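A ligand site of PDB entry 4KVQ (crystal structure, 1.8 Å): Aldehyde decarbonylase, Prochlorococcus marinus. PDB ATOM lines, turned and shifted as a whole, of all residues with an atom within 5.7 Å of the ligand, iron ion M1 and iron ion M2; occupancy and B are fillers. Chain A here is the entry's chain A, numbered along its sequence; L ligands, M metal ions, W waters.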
ATOM      1  N   TYR A  35      20.677  -0.053 -11.517  1.00  0.00           N
ATOM      2  CA  TYR A  35      20.036  -0.250 -12.826  1.00  0.00           C
ATOM      3  C   TYR A  35      18.655   0.395 -12.839  1.00  0.00           C
ATOM      4  O   TYR A  35      18.217   0.875 -13.880  1.00  0.00           O
ATOM      5  CB  TYR A  35      19.950  -1.737 -13.179  1.00  0.00           C
ATOM      6  CG  TYR A  35      19.896  -1.996 -14.691  1.00  0.00           C
ATOM      7  CD1 TYR A  35      21.056  -2.035 -15.449  1.00  0.00           C
ATOM      8  CD2 TYR A  35      18.679  -2.189 -15.347  1.00  0.00           C
ATOM      9  CE1 TYR A  35      21.016  -2.253 -16.827  1.00  0.00           C
ATOM     10  CE2 TYR A  35      18.629  -2.424 -16.718  1.00  0.00           C
ATOM     11  CZ  TYR A  35      19.802  -2.450 -17.450  1.00  0.00           C
ATOM     12  OH  TYR A  35      19.770  -2.685 -18.808  1.00  0.00           O
ATOM     13  N   ILE A  38      19.450   3.997 -13.850  1.00  0.00           N
ATOM     14  CA  ILE A  38      20.061   4.100 -15.183  1.00  0.00           C
ATOM     15  C   ILE A  38      19.066   3.688 -16.281  1.00  0.00           C
ATOM     16  O   ILE A  38      18.929   4.366 -17.303  1.00  0.00           O
ATOM     17  CB  ILE A  38      21.294   3.205 -15.292  1.00  0.00           C
ATOM     18  CG1 ILE A  38      22.385   3.692 -14.351  1.00  0.00           C
ATOM     19  CG2 ILE A  38      21.835   3.162 -16.742  1.00  0.00           C
ATOM     20  CD1 ILE A  38      22.793   5.072 -14.627  1.00  0.00           C
ATOM     21  N   ILE A  41      16.503   6.423 -16.744  1.00  0.00           N
ATOM     22  CA  ILE A  41      17.051   7.559 -17.485  1.00  0.00           C
ATOM     23  C   ILE A  41      17.067   7.285 -18.986  1.00  0.00           C
ATOM     24  O   ILE A  41      16.682   8.149 -19.773  1.00  0.00           O
ATOM     25  CB  ILE A  41      18.484   7.909 -16.978  1.00  0.00           C
ATOM     26  CG1 ILE A  41      18.387   8.615 -15.623  1.00  0.00           C
ATOM     27  CG2 ILE A  41      19.217   8.800 -17.971  1.00  0.00           C
ATOM     28  CD1 ILE A  41      19.734   8.811 -14.931  1.00  0.00           C
ATOM     29  N   VAL A  42      17.478   6.089 -19.371  1.00  0.00           N
ATOM     30  CA  VAL A  42      17.494   5.736 -20.795  1.00  0.00           C
ATOM     31  C   VAL A  42      16.062   5.710 -21.375  1.00  0.00           C
ATOM     32  O   VAL A  42      15.810   6.248 -22.447  1.00  0.00           O
ATOM     33  CB  VAL A  42      18.234   4.401 -21.023  1.00  0.00           C
ATOM     34  CG1 VAL A  42      18.114   3.990 -22.451  1.00  0.00           C
ATOM     35  CG2 VAL A  42      19.717   4.542 -20.638  1.00  0.00           C
ATOM     36  N   GLY A  45      14.886   9.209 -21.682  1.00  0.00           N
ATOM     37  CA  GLY A  45      15.617   9.890 -22.717  1.00  0.00           C
ATOM     38  C   GLY A  45      15.101   9.535 -24.103  1.00  0.00           C
ATOM     39  O   GLY A  45      15.025  10.405 -24.976  1.00  0.00           O
ATOM     40  N   GLU A  46      14.796   8.266 -24.317  1.00  0.00           N
ATOM     41  CA  GLU A  46      14.247   7.821 -25.597  1.00  0.00           C
ATOM     42  C   GLU A  46      12.882   8.434 -25.850  1.00  0.00           C
ATOM     43  O   GLU A  46      12.577   8.829 -26.957  1.00  0.00           O
ATOM     44  CB  GLU A  46      14.169   6.290 -25.657  1.00  0.00           C
ATOM     45  CG  GLU A  46      15.518   5.591 -25.499  1.00  0.00           C
ATOM     46  CD  GLU A  46      16.431   5.787 -26.701  1.00  0.00           C
ATOM     47  OE1 GLU A  46      15.953   6.325 -27.729  1.00  0.00           O
ATOM     48  OE2 GLU A  46      17.620   5.407 -26.625  1.00  0.00           O
ATOM     49  N   ALA A  49      13.485  11.983 -26.748  1.00  0.00           N
ATOM     50  CA  ALA A  49      14.010  12.068 -28.115  1.00  0.00           C
ATOM     51  C   ALA A  49      12.847  11.987 -29.102  1.00  0.00           C
ATOM     52  O   ALA A  49      12.760  12.786 -30.040  1.00  0.00           O
ATOM     53  CB  ALA A  49      15.046  10.964 -28.371  1.00  0.00           C
ATOM     54  N   TYR A  53      11.913  15.141 -31.685  1.00  0.00           N
ATOM     55  CA  TYR A  53      11.900  15.092 -33.141  1.00  0.00           C
ATOM     56  C   TYR A  53      10.509  15.454 -33.687  1.00  0.00           C
ATOM     57  O   TYR A  53      10.410  16.152 -34.686  1.00  0.00           O
ATOM     58  CB  TYR A  53      12.389  13.740 -33.681  1.00  0.00           C
ATOM     59  CG  TYR A  53      13.880  13.577 -33.522  1.00  0.00           C
ATOM     60  CD1 TYR A  53      14.762  14.494 -34.089  1.00  0.00           C
ATOM     61  CD2 TYR A  53      14.422  12.513 -32.800  1.00  0.00           C
ATOM     62  CE1 TYR A  53      16.139  14.361 -33.944  1.00  0.00           C
ATOM     63  CE2 TYR A  53      15.808  12.378 -32.660  1.00  0.00           C
ATOM     64  CZ  TYR A  53      16.647  13.310 -33.229  1.00  0.00           C
ATOM     65  OH  TYR A  53      18.015  13.178 -33.080  1.00  0.00           O
ATOM     66  N   MET A  73      11.805   5.451 -34.483  1.00  0.00           N
ATOM     67  CA  MET A  73      12.978   4.705 -34.042  1.00  0.00           C
ATOM     68  C   MET A  73      13.166   4.867 -32.539  1.00  0.00           C
ATOM     69  O   MET A  73      13.513   3.910 -31.845  1.00  0.00           O
ATOM     70  CB  MET A  73      14.263   5.149 -34.761  1.00  0.00           C
ATOM     71  CG  MET A  73      14.278   4.955 -36.271  1.00  0.00           C
ATOM     72  SD  MET A  73      15.861   5.505 -36.970  1.00  0.00           S
ATOM     73  CE  MET A  73      15.424   5.602 -38.717  1.00  0.00           C
ATOM     74  N   GLU A  74      12.967   6.090 -32.048  1.00  0.00           N
ATOM     75  CA  GLU A  74      13.150   6.362 -30.624  1.00  0.00           C
ATOM     76  C   GLU A  74      12.167   5.538 -29.806  1.00  0.00           C
ATOM     77  O   GLU A  74      12.501   5.055 -28.725  1.00  0.00           O
ATOM     78  CB  GLU A  74      13.008   7.857 -30.305  1.00  0.00           C
ATOM     79  CG  GLU A  74      13.959   8.778 -31.107  1.00  0.00           C
ATOM     80  CD  GLU A  74      15.450   8.554 -30.829  1.00  0.00           C
ATOM     81  OE1 GLU A  74      15.835   7.491 -30.321  1.00  0.00           O
ATOM     82  OE2 GLU A  74      16.254   9.459 -31.153  1.00  0.00           O
ATOM     83  N   HIS A  77      13.533   2.088 -29.520  1.00  0.00           N
ATOM     84  CA  HIS A  77      14.609   2.058 -28.510  1.00  0.00           C
ATOM     85  C   HIS A  77      13.998   2.019 -27.106  1.00  0.00           C
ATOM     86  O   HIS A  77      14.437   1.264 -26.246  1.00  0.00           O
ATOM     87  CB  HIS A  77      15.495   3.306 -28.624  1.00  0.00           C
ATOM     88  CG  HIS A  77      16.114   3.497 -29.972  1.00  0.00           C
ATOM     89  ND1 HIS A  77      16.772   4.656 -30.323  1.00  0.00           N
ATOM     90  CD2 HIS A  77      16.199   2.676 -31.049  1.00  0.00           C
ATOM     91  CE1 HIS A  77      17.222   4.556 -31.564  1.00  0.00           C
ATOM     92  NE2 HIS A  77      16.880   3.361 -32.026  1.00  0.00           N
ATOM     93  N   PHE A  81      14.669  -0.878 -24.300  1.00  0.00           N
ATOM     94  CA  PHE A  81      15.292  -0.640 -22.999  1.00  0.00           C
ATOM     95  C   PHE A  81      14.323  -0.913 -21.861  1.00  0.00           C
ATOM     96  O   PHE A  81      14.721  -1.342 -20.784  1.00  0.00           O
ATOM     97  CB  PHE A  81      15.871   0.778 -22.949  1.00  0.00           C
ATOM     98  CG  PHE A  81      17.090   0.961 -23.806  1.00  0.00           C
ATOM     99  CD1 PHE A  81      18.158   0.081 -23.679  1.00  0.00           C
ATOM    100  CD2 PHE A  81      17.176   1.967 -24.742  1.00  0.00           C
ATOM    101  CE1 PHE A  81      19.299   0.221 -24.471  1.00  0.00           C
ATOM    102  CE2 PHE A  81      18.324   2.128 -25.528  1.00  0.00           C
ATOM    103  CZ  PHE A  81      19.373   1.251 -25.392  1.00  0.00           C
ATOM    104  N   PHE A 100      16.116  14.183 -13.787  1.00  0.00           N
ATOM    105  CA  PHE A 100      17.428  14.166 -14.442  1.00  0.00           C
ATOM    106  C   PHE A 100      17.416  14.958 -15.741  1.00  0.00           C
ATOM    107  O   PHE A 100      18.365  15.691 -16.027  1.00  0.00           O
ATOM    108  CB  PHE A 100      17.811  12.706 -14.716  1.00  0.00           C
ATOM    109  CG  PHE A 100      19.151  12.515 -15.364  1.00  0.00           C
ATOM    110  CD1 PHE A 100      20.327  12.544 -14.614  1.00  0.00           C
ATOM    111  CD2 PHE A 100      19.243  12.227 -16.721  1.00  0.00           C
ATOM    112  CE1 PHE A 100      21.551  12.322 -15.212  1.00  0.00           C
ATOM    113  CE2 PHE A 100      20.467  12.004 -17.320  1.00  0.00           C
ATOM    114  CZ  PHE A 100      21.626  12.037 -16.561  1.00  0.00           C
ATOM    115  N   PHE A 101      16.361  14.787 -16.536  1.00  0.00           N
ATOM    116  CA  PHE A 101      16.225  15.448 -17.836  1.00  0.00           C
ATOM    117  C   PHE A 101      15.588  16.834 -17.788  1.00  0.00           C
ATOM    118  O   PHE A 101      15.625  17.549 -18.788  1.00  0.00           O
ATOM    119  CB  PHE A 101      15.440  14.577 -18.814  1.00  0.00           C
ATOM    120  CG  PHE A 101      16.286  13.546 -19.479  1.00  0.00           C
ATOM    121  CD1 PHE A 101      17.135  13.911 -20.501  1.00  0.00           C
ATOM    122  CD2 PHE A 101      16.253  12.222 -19.070  1.00  0.00           C
ATOM    123  CE1 PHE A 101      17.943  12.964 -21.112  1.00  0.00           C
ATOM    124  CE2 PHE A 101      17.066  11.286 -19.674  1.00  0.00           C
ATOM    125  CZ  PHE A 101      17.906  11.652 -20.692  1.00  0.00           C
ATOM    126  N   GLN A 124      19.019  18.225 -29.185  1.00  0.00           N
ATOM    127  CA  GLN A 124      18.629  16.838 -29.367  1.00  0.00           C
ATOM    128  C   GLN A 124      19.578  16.072 -30.270  1.00  0.00           C
ATOM    129  O   GLN A 124      20.108  15.037 -29.870  1.00  0.00           O
ATOM    130  CB  GLN A 124      17.209  16.702 -29.928  1.00  0.00           C
ATOM    131  CG  GLN A 124      16.883  15.231 -30.322  1.00  0.00           C
ATOM    132  CD  GLN A 124      16.927  14.272 -29.153  1.00  0.00           C
ATOM    133  OE1 GLN A 124      16.414  14.566 -28.072  1.00  0.00           O
ATOM    134  NE2 GLN A 124      17.547  13.095 -29.364  1.00  0.00           N
ATOM    135  N   ILE A 128      22.363  15.390 -27.099  1.00  0.00           N
ATOM    136  CA  ILE A 128      21.728  14.201 -26.544  1.00  0.00           C
ATOM    137  C   ILE A 128      22.097  12.943 -27.328  1.00  0.00           C
ATOM    138  O   ILE A 128      22.390  11.915 -26.722  1.00  0.00           O
ATOM    139  CB  ILE A 128      20.210  14.379 -26.389  1.00  0.00           C
ATOM    140  CG1 ILE A 128      19.928  15.476 -25.360  1.00  0.00           C
ATOM    141  CG2 ILE A 128      19.572  13.080 -25.943  1.00  0.00           C
ATOM    142  CD1 ILE A 128      18.461  15.787 -25.168  1.00  0.00           C
ATOM    143  N   GLU A 129      22.142  13.010 -28.659  1.00  0.00           N
ATOM    144  CA  GLU A 129      22.545  11.833 -29.424  1.00  0.00           C
ATOM    145  C   GLU A 129      23.998  11.444 -29.118  1.00  0.00           C
ATOM    146  O   GLU A 129      24.290  10.270 -28.954  1.00  0.00           O
ATOM    147  CB  GLU A 129      22.381  12.013 -30.934  1.00  0.00           C
ATOM    148  CG  GLU A 129      20.962  12.289 -31.411  1.00  0.00           C
ATOM    149  CD  GLU A 129      20.009  11.103 -31.271  1.00  0.00           C
ATOM    150  OE1 GLU A 129      20.465   9.952 -31.056  1.00  0.00           O
ATOM    151  OE2 GLU A 129      18.770  11.314 -31.414  1.00  0.00           O
ATOM    152  N   PHE A 131      25.606  11.998 -26.321  1.00  0.00           N
ATOM    153  CA  PHE A 131      25.597  11.474 -24.954  1.00  0.00           C
ATOM    154  C   PHE A 131      25.129  10.008 -24.986  1.00  0.00           C
ATOM    155  O   PHE A 131      25.733   9.133 -24.373  1.00  0.00           O
ATOM    156  CB  PHE A 131      24.665  12.352 -24.106  1.00  0.00           C
ATOM    157  CG  PHE A 131      24.664  12.029 -22.632  1.00  0.00           C
ATOM    158  CD1 PHE A 131      25.670  11.270 -22.062  1.00  0.00           C
ATOM    159  CD2 PHE A 131      23.638  12.491 -21.822  1.00  0.00           C
ATOM    160  CE1 PHE A 131      25.657  10.981 -20.698  1.00  0.00           C
ATOM    161  CE2 PHE A 131      23.612  12.202 -20.463  1.00  0.00           C
ATOM    162  CZ  PHE A 131      24.623  11.441 -19.907  1.00  0.00           C
ATOM    163  N   ALA A 132      24.066   9.752 -25.744  1.00  0.00           N
ATOM    164  CA  ALA A 132      23.543   8.395 -25.885  1.00  0.00           C
ATOM    165  C   ALA A 132      24.555   7.454 -26.519  1.00  0.00           C
ATOM    166  O   ALA A 132      24.775   6.351 -26.037  1.00  0.00           O
ATOM    167  CB  ALA A 132      22.268   8.403 -26.716  1.00  0.00           C
ATOM    168  N   ALA A 135      27.312   6.687 -24.109  1.00  0.00           N
ATOM    169  CA  ALA A 135      26.807   5.839 -23.031  1.00  0.00           C
ATOM    170  C   ALA A 135      26.569   4.415 -23.518  1.00  0.00           C
ATOM    171  O   ALA A 135      26.983   3.454 -22.868  1.00  0.00           O
ATOM    172  CB  ALA A 135      25.538   6.425 -22.475  1.00  0.00           C
ATOM    173  N   TYR A 136      25.907   4.280 -24.656  1.00  0.00           N
ATOM    174  CA  TYR A 136      25.628   2.938 -25.166  1.00  0.00           C
ATOM    175  C   TYR A 136      26.898   2.179 -25.533  1.00  0.00           C
ATOM    176  O   TYR A 136      27.016   0.994 -25.238  1.00  0.00           O
ATOM    177  CB  TYR A 136      24.646   3.010 -26.350  1.00  0.00           C
ATOM    178  CG  TYR A 136      23.297   3.602 -25.991  1.00  0.00           C
ATOM    179  CD1 TYR A 136      22.871   3.683 -24.669  1.00  0.00           C
ATOM    180  CD2 TYR A 136      22.459   4.100 -26.982  1.00  0.00           C
ATOM    181  CE1 TYR A 136      21.636   4.239 -24.340  1.00  0.00           C
ATOM    182  CE2 TYR A 136      21.212   4.666 -26.659  1.00  0.00           C
ATOM    183  CZ  TYR A 136      20.824   4.722 -25.342  1.00  0.00           C
ATOM    184  OH  TYR A 136      19.608   5.284 -25.023  1.00  0.00           O
ATOM    185  N   TYR A 139      28.469   0.983 -22.320  1.00  0.00           N
ATOM    186  CA  TYR A 139      27.681  -0.049 -21.652  1.00  0.00           C
ATOM    187  C   TYR A 139      27.794  -1.415 -22.319  1.00  0.00           C
ATOM    188  O   TYR A 139      27.789  -2.431 -21.635  1.00  0.00           O
ATOM    189  CB  TYR A 139      26.221   0.389 -21.612  1.00  0.00           C
ATOM    190  CG  TYR A 139      25.213  -0.628 -21.107  1.00  0.00           C
ATOM    191  CD1 TYR A 139      25.283  -1.142 -19.814  1.00  0.00           C
ATOM    192  CD2 TYR A 139      24.120  -1.010 -21.902  1.00  0.00           C
ATOM    193  CE1 TYR A 139      24.337  -2.038 -19.342  1.00  0.00           C
ATOM    194  CE2 TYR A 139      23.166  -1.904 -21.426  1.00  0.00           C
ATOM    195  CZ  TYR A 139      23.281  -2.416 -20.155  1.00  0.00           C
ATOM    196  OH  TYR A 139      22.332  -3.303 -19.694  1.00  0.00           O
ATOM    197  N   THR A 151      21.062  -3.099 -27.120  1.00  0.00           N
ATOM    198  CA  THR A 151      21.871  -1.901 -27.213  1.00  0.00           C
ATOM    199  C   THR A 151      22.684  -1.833 -28.507  1.00  0.00           C
ATOM    200  O   THR A 151      22.831  -0.765 -29.099  1.00  0.00           O
ATOM    201  CB  THR A 151      22.810  -1.759 -25.988  1.00  0.00           C
ATOM    202  OG1 THR A 151      22.058  -1.959 -24.775  1.00  0.00           O
ATOM    203  CG2 THR A 151      23.450  -0.372 -25.964  1.00  0.00           C
ATOM    204  N   VAL A 154      20.427  -0.534 -31.148  1.00  0.00           N
ATOM    205  CA  VAL A 154      20.102   0.889 -31.000  1.00  0.00           C
ATOM    206  C   VAL A 154      21.213   1.817 -31.490  1.00  0.00           C
ATOM    207  O   VAL A 154      20.940   2.851 -32.106  1.00  0.00           O
ATOM    208  CB  VAL A 154      19.772   1.211 -29.519  1.00  0.00           C
ATOM    209  CG1 VAL A 154      19.847   2.714 -29.264  1.00  0.00           C
ATOM    210  CG2 VAL A 154      18.386   0.669 -29.142  1.00  0.00           C
ATOM    211  N   ASP A 157      21.223   3.253 -35.006  1.00  0.00           N
ATOM    212  CA  ASP A 157      20.217   4.280 -35.249  1.00  0.00           C
ATOM    213  C   ASP A 157      20.688   5.645 -34.792  1.00  0.00           C
ATOM    214  O   ASP A 157      20.346   6.666 -35.406  1.00  0.00           O
ATOM    215  CB  ASP A 157      18.900   3.972 -34.530  1.00  0.00           C
ATOM    216  CG  ASP A 157      18.092   2.888 -35.214  1.00  0.00           C
ATOM    217  OD1 ASP A 157      18.438   2.528 -36.362  1.00  0.00           O
ATOM    218  OD2 ASP A 157      17.108   2.426 -34.607  1.00  0.00           O
ATOM    219  N   GLU A 158      21.447   5.701 -33.703  1.00  0.00           N
ATOM    220  CA  GLU A 158      21.781   7.022 -33.162  1.00  0.00           C
ATOM    221  C   GLU A 158      22.784   7.745 -34.089  1.00  0.00           C
ATOM    222  O   GLU A 158      22.795   8.976 -34.152  1.00  0.00           O
ATOM    223  CB  GLU A 158      22.224   6.972 -31.681  1.00  0.00           C
ATOM    224  CG  GLU A 158      21.367   6.033 -30.744  1.00  0.00           C
ATOM    225  CD  GLU A 158      19.910   6.481 -30.393  1.00  0.00           C
ATOM    226  OE1 GLU A 158      19.407   6.030 -29.318  1.00  0.00           O
ATOM    227  OE2 GLU A 158      19.240   7.236 -31.150  1.00  0.00           O
ATOM    228  N   HIS A 161      20.799   9.602 -36.460  1.00  0.00           N
ATOM    229  CA  HIS A 161      20.172  10.780 -35.887  1.00  0.00           C
ATOM    230  C   HIS A 161      21.165  11.920 -35.851  1.00  0.00           C
ATOM    231  O   HIS A 161      20.842  13.054 -36.207  1.00  0.00           O
ATOM    232  CB  HIS A 161      19.641  10.446 -34.487  1.00  0.00           C
ATOM    233  CG  HIS A 161      18.570   9.402 -34.486  1.00  0.00           C
ATOM    234  ND1 HIS A 161      18.057   8.873 -33.329  1.00  0.00           N
ATOM    235  CD2 HIS A 161      17.928   8.797 -35.499  1.00  0.00           C
ATOM    236  CE1 HIS A 161      17.138   7.976 -33.633  1.00  0.00           C
ATOM    237  NE2 HIS A 161      17.040   7.907 -34.955  1.00  0.00           N
ATOM    238  N   VAL A 198      25.189  10.822 -13.127  1.00  0.00           N
ATOM    239  CA  VAL A 198      24.996   9.426 -13.483  1.00  0.00           C
ATOM    240  C   VAL A 198      26.208   8.564 -13.103  1.00  0.00           C
ATOM    241  O   VAL A 198      26.124   7.328 -13.050  1.00  0.00           O
ATOM    242  CB  VAL A 198      24.669   9.327 -14.992  1.00  0.00           C
ATOM    243  CG1 VAL A 198      25.920   9.053 -15.823  1.00  0.00           C
ATOM    244  CG2 VAL A 198      23.602   8.300 -15.252  1.00  0.00           C
ATOM    245  N   ALA A 202      26.543   4.535 -12.812  1.00  0.00           N
ATOM    246  CA  ALA A 202      27.274   3.976 -13.947  1.00  0.00           C
ATOM    247  C   ALA A 202      28.445   3.120 -13.492  1.00  0.00           C
ATOM    248  O   ALA A 202      28.733   2.092 -14.106  1.00  0.00           O
ATOM    249  CB  ALA A 202      27.744   5.090 -14.917  1.00  0.00           C
ATOM    250  N   LEU A 205      27.509  -0.245 -12.608  1.00  0.00           N
ATOM    251  CA  LEU A 205      27.317  -0.985 -13.850  1.00  0.00           C
ATOM    252  C   LEU A 205      28.637  -1.307 -14.563  1.00  0.00           C
ATOM    253  O   LEU A 205      28.632  -1.812 -15.689  1.00  0.00           O
ATOM    254  CB  LEU A 205      26.373  -0.223 -14.787  1.00  0.00           C
ATOM    255  CG  LEU A 205      24.869  -0.514 -14.684  1.00  0.00           C
ATOM    256  CD1 LEU A 205      24.314  -0.266 -13.296  1.00  0.00           C
ATOM    257  CD2 LEU A 205      24.121   0.349 -15.695  1.00  0.00           C
ATOM    258  N   MET A 207      30.903   0.848 -15.610  1.00  0.00           N
ATOM    259  CA  MET A 207      31.241   1.837 -16.623  1.00  0.00           C
ATOM    260  C   MET A 207      32.127   2.931 -16.013  1.00  0.00           C
ATOM    261  O   MET A 207      31.800   3.466 -14.962  1.00  0.00           O
ATOM    262  CB  MET A 207      29.959   2.453 -17.175  1.00  0.00           C
ATOM    263  CG  MET A 207      29.053   1.417 -17.872  1.00  0.00           C
ATOM    264  SD  MET A 207      27.404   2.083 -18.226  1.00  0.00           S
ATOM    265  CE  MET A 207      27.843   3.282 -19.437  1.00  0.00           C
ATOM    266  N   LEU A 212      33.033   7.577 -20.509  1.00  0.00           N
ATOM    267  CA  LEU A 212      31.795   8.274 -20.857  1.00  0.00           C
ATOM    268  C   LEU A 212      32.082   9.694 -21.335  1.00  0.00           C
ATOM    269  O   LEU A 212      31.568  10.144 -22.357  1.00  0.00           O
ATOM    270  CB  LEU A 212      30.837   8.304 -19.670  1.00  0.00           C
ATOM    271  CG  LEU A 212      30.116   7.014 -19.285  1.00  0.00           C
ATOM    272  CD1 LEU A 212      29.313   7.189 -17.991  1.00  0.00           C
ATOM    273  CD2 LEU A 212      29.192   6.580 -20.415  1.00  0.00           C
HETATM  274  C1  LIG L   1      18.266   9.271 -28.288  1.00  0.00           C
HETATM  275  O1  LIG L   1      17.955   8.491 -29.175  1.00  0.00           O
HETATM  276  O2  LIG L   1      18.569  10.487 -28.392  1.00  0.00           O
HETATM  277  C2  LIG L   1      18.300   8.651 -26.864  1.00  0.00           C
HETATM  278  C3  LIG L   1      18.752   9.586 -25.762  1.00  0.00           C
HETATM  279  C4  LIG L   1      18.856   8.933 -24.368  1.00  0.00           C
HETATM  280  C5  LIG L   1      19.998   9.474 -23.504  1.00  0.00           C
HETATM  281  C6  LIG L   1      20.604   8.421 -22.557  1.00  0.00           C
HETATM  282  C7  LIG L   1      21.777   8.906 -21.701  1.00  0.00           C
HETATM  283  C8  LIG L   1      21.950   8.111 -20.392  1.00  0.00           C
HETATM  284  C9  LIG L   1      23.398   7.839 -19.997  1.00  0.00           C
HETATM  285  C10 LIG L   1      23.549   6.990 -18.714  1.00  0.00           C
HETATM  286  C11 LIG L   1      24.249   5.622 -18.919  1.00  0.00           C
HETATM  287  C12 LIG L   1      23.341   4.605 -19.629  1.00  0.00           C
HETATM  288  C13 LIG L   1      24.038   3.310 -20.009  1.00  0.00           C
HETATM  289  C14 LIG L   1      23.232   2.486 -21.027  1.00  0.00           C
HETATM  290  C15 LIG L   1      22.182   1.577 -20.391  1.00  0.00           C
HETATM  291  C16 LIG L   1      21.238   0.996 -21.437  1.00  0.00           C
HETATM  292 FE    FE M   1      17.300   6.547 -29.305  1.00  0.00          FE
HETATM  293 FE    FE M   2      18.303   9.189 -31.122  1.00  0.00          FE
HETATM  294  O   HOH W   1      18.780   0.225 -19.966  1.00  0.00           O
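Four residues have an atom within 4 Å of iron ion M1: Glu 46, Glu 74, His 77 and Glu 158.
Within 4 Å of iron ion M2: Glu 74, Glu 129, Glu 158 and His 161.
The side-chain amide nitrogen of Gln 124 lies within hydrogen-bond range of an oxygen (O2) of the ligand (3.0 Å).
Residues that only touch the ligand: Ile 38 (3.6 Å), Ile 41 (3.7 Å), Val 42 (3.8 Å), Gly 45 (3.8 Å), Ala 49 (3.6 Å), Phe 81 (3.7 Å), Ile 128 (3.6 Å), Phe 131 (3.8 Å), Ala 132 (3.8 Å), Ala 135 (3.6 Å), Tyr 136 (3.8 Å), Tyr 139 (3.5 Å), Val 198 (3.7 Å) and Met 207 (3.8 Å). 19 residues have an atom within 4 Å of the ligand: Ile 38, Ile 41, Val 42, Gly 45, Glu 46, Ala 49, Glu 74, Phe 81, Gln 124, Ile 128, Glu 129, Phe 131, Ala 132, Ala 135, Tyr 136, Tyr 139, Glu 158, Val 198 and Met 207. The nearest printed residue that does not touch the ligand is Phe 101 (4.1 Å).
Iron ion M2 is bound by the side-chain carboxylate (OE2) of Glu 74, an oxygen (O1) of the ligand, the side-chain carboxylate (OE2) of Glu 158, the side-chain carboxylate (OE2) of Glu 129, a ring nitrogen (ND1) of His 161 and the side-chain carboxylate (OE1) of Glu 129.
Iron ion M1 is bound by OE1 of Glu 74 (2.0 Å). Iron ion M1 is bound by O1 of the ligand (2.1 Å). OE1 of Glu 46 binds iron ion M1 (2.1 Å). OE1 of Glu 158 binds iron ion M1 (2.2 Å). A ring nitrogen (ND1) of His 77 is bound to iron ion M1 (2.2 Å). Iron ion M1 has five donor atoms within binding distance. Slightly farther from iron ion M1 lies the side-chain carboxylate (OE2) of Glu 158 (2.8 Å).
OH of Tyr 136 lies within hydrogen-bond range of OE2 of Glu 46 (2.6 Å). N of Glu 129 is in hydrogen-bond range of O of Gln 124 (3.1 Å). OE2 of Glu 129 lies close to OH of Tyr 53 (2.6 Å). A ring nitrogen (NE2) of His 77 lies close to the backbone carbonyl oxygen (O) of Met 73 (3.4 Å). NE2 of His 77 sits at hydrogen-bond distance from OD2 of Asp 157, 2.8 Å away. A ring nitrogen (NE2) of His 161 sits at hydrogen-bond distance from the side-chain sulfur (SD) of Met 73, at 3.3 Å. The side-chain hydroxyl of Tyr 139 is in hydrogen-bond range of the side-chain hydroxyl of Tyr 35 (2.8 Å). O of Ala 202 is in hydrogen-bond range of N of Met 207.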
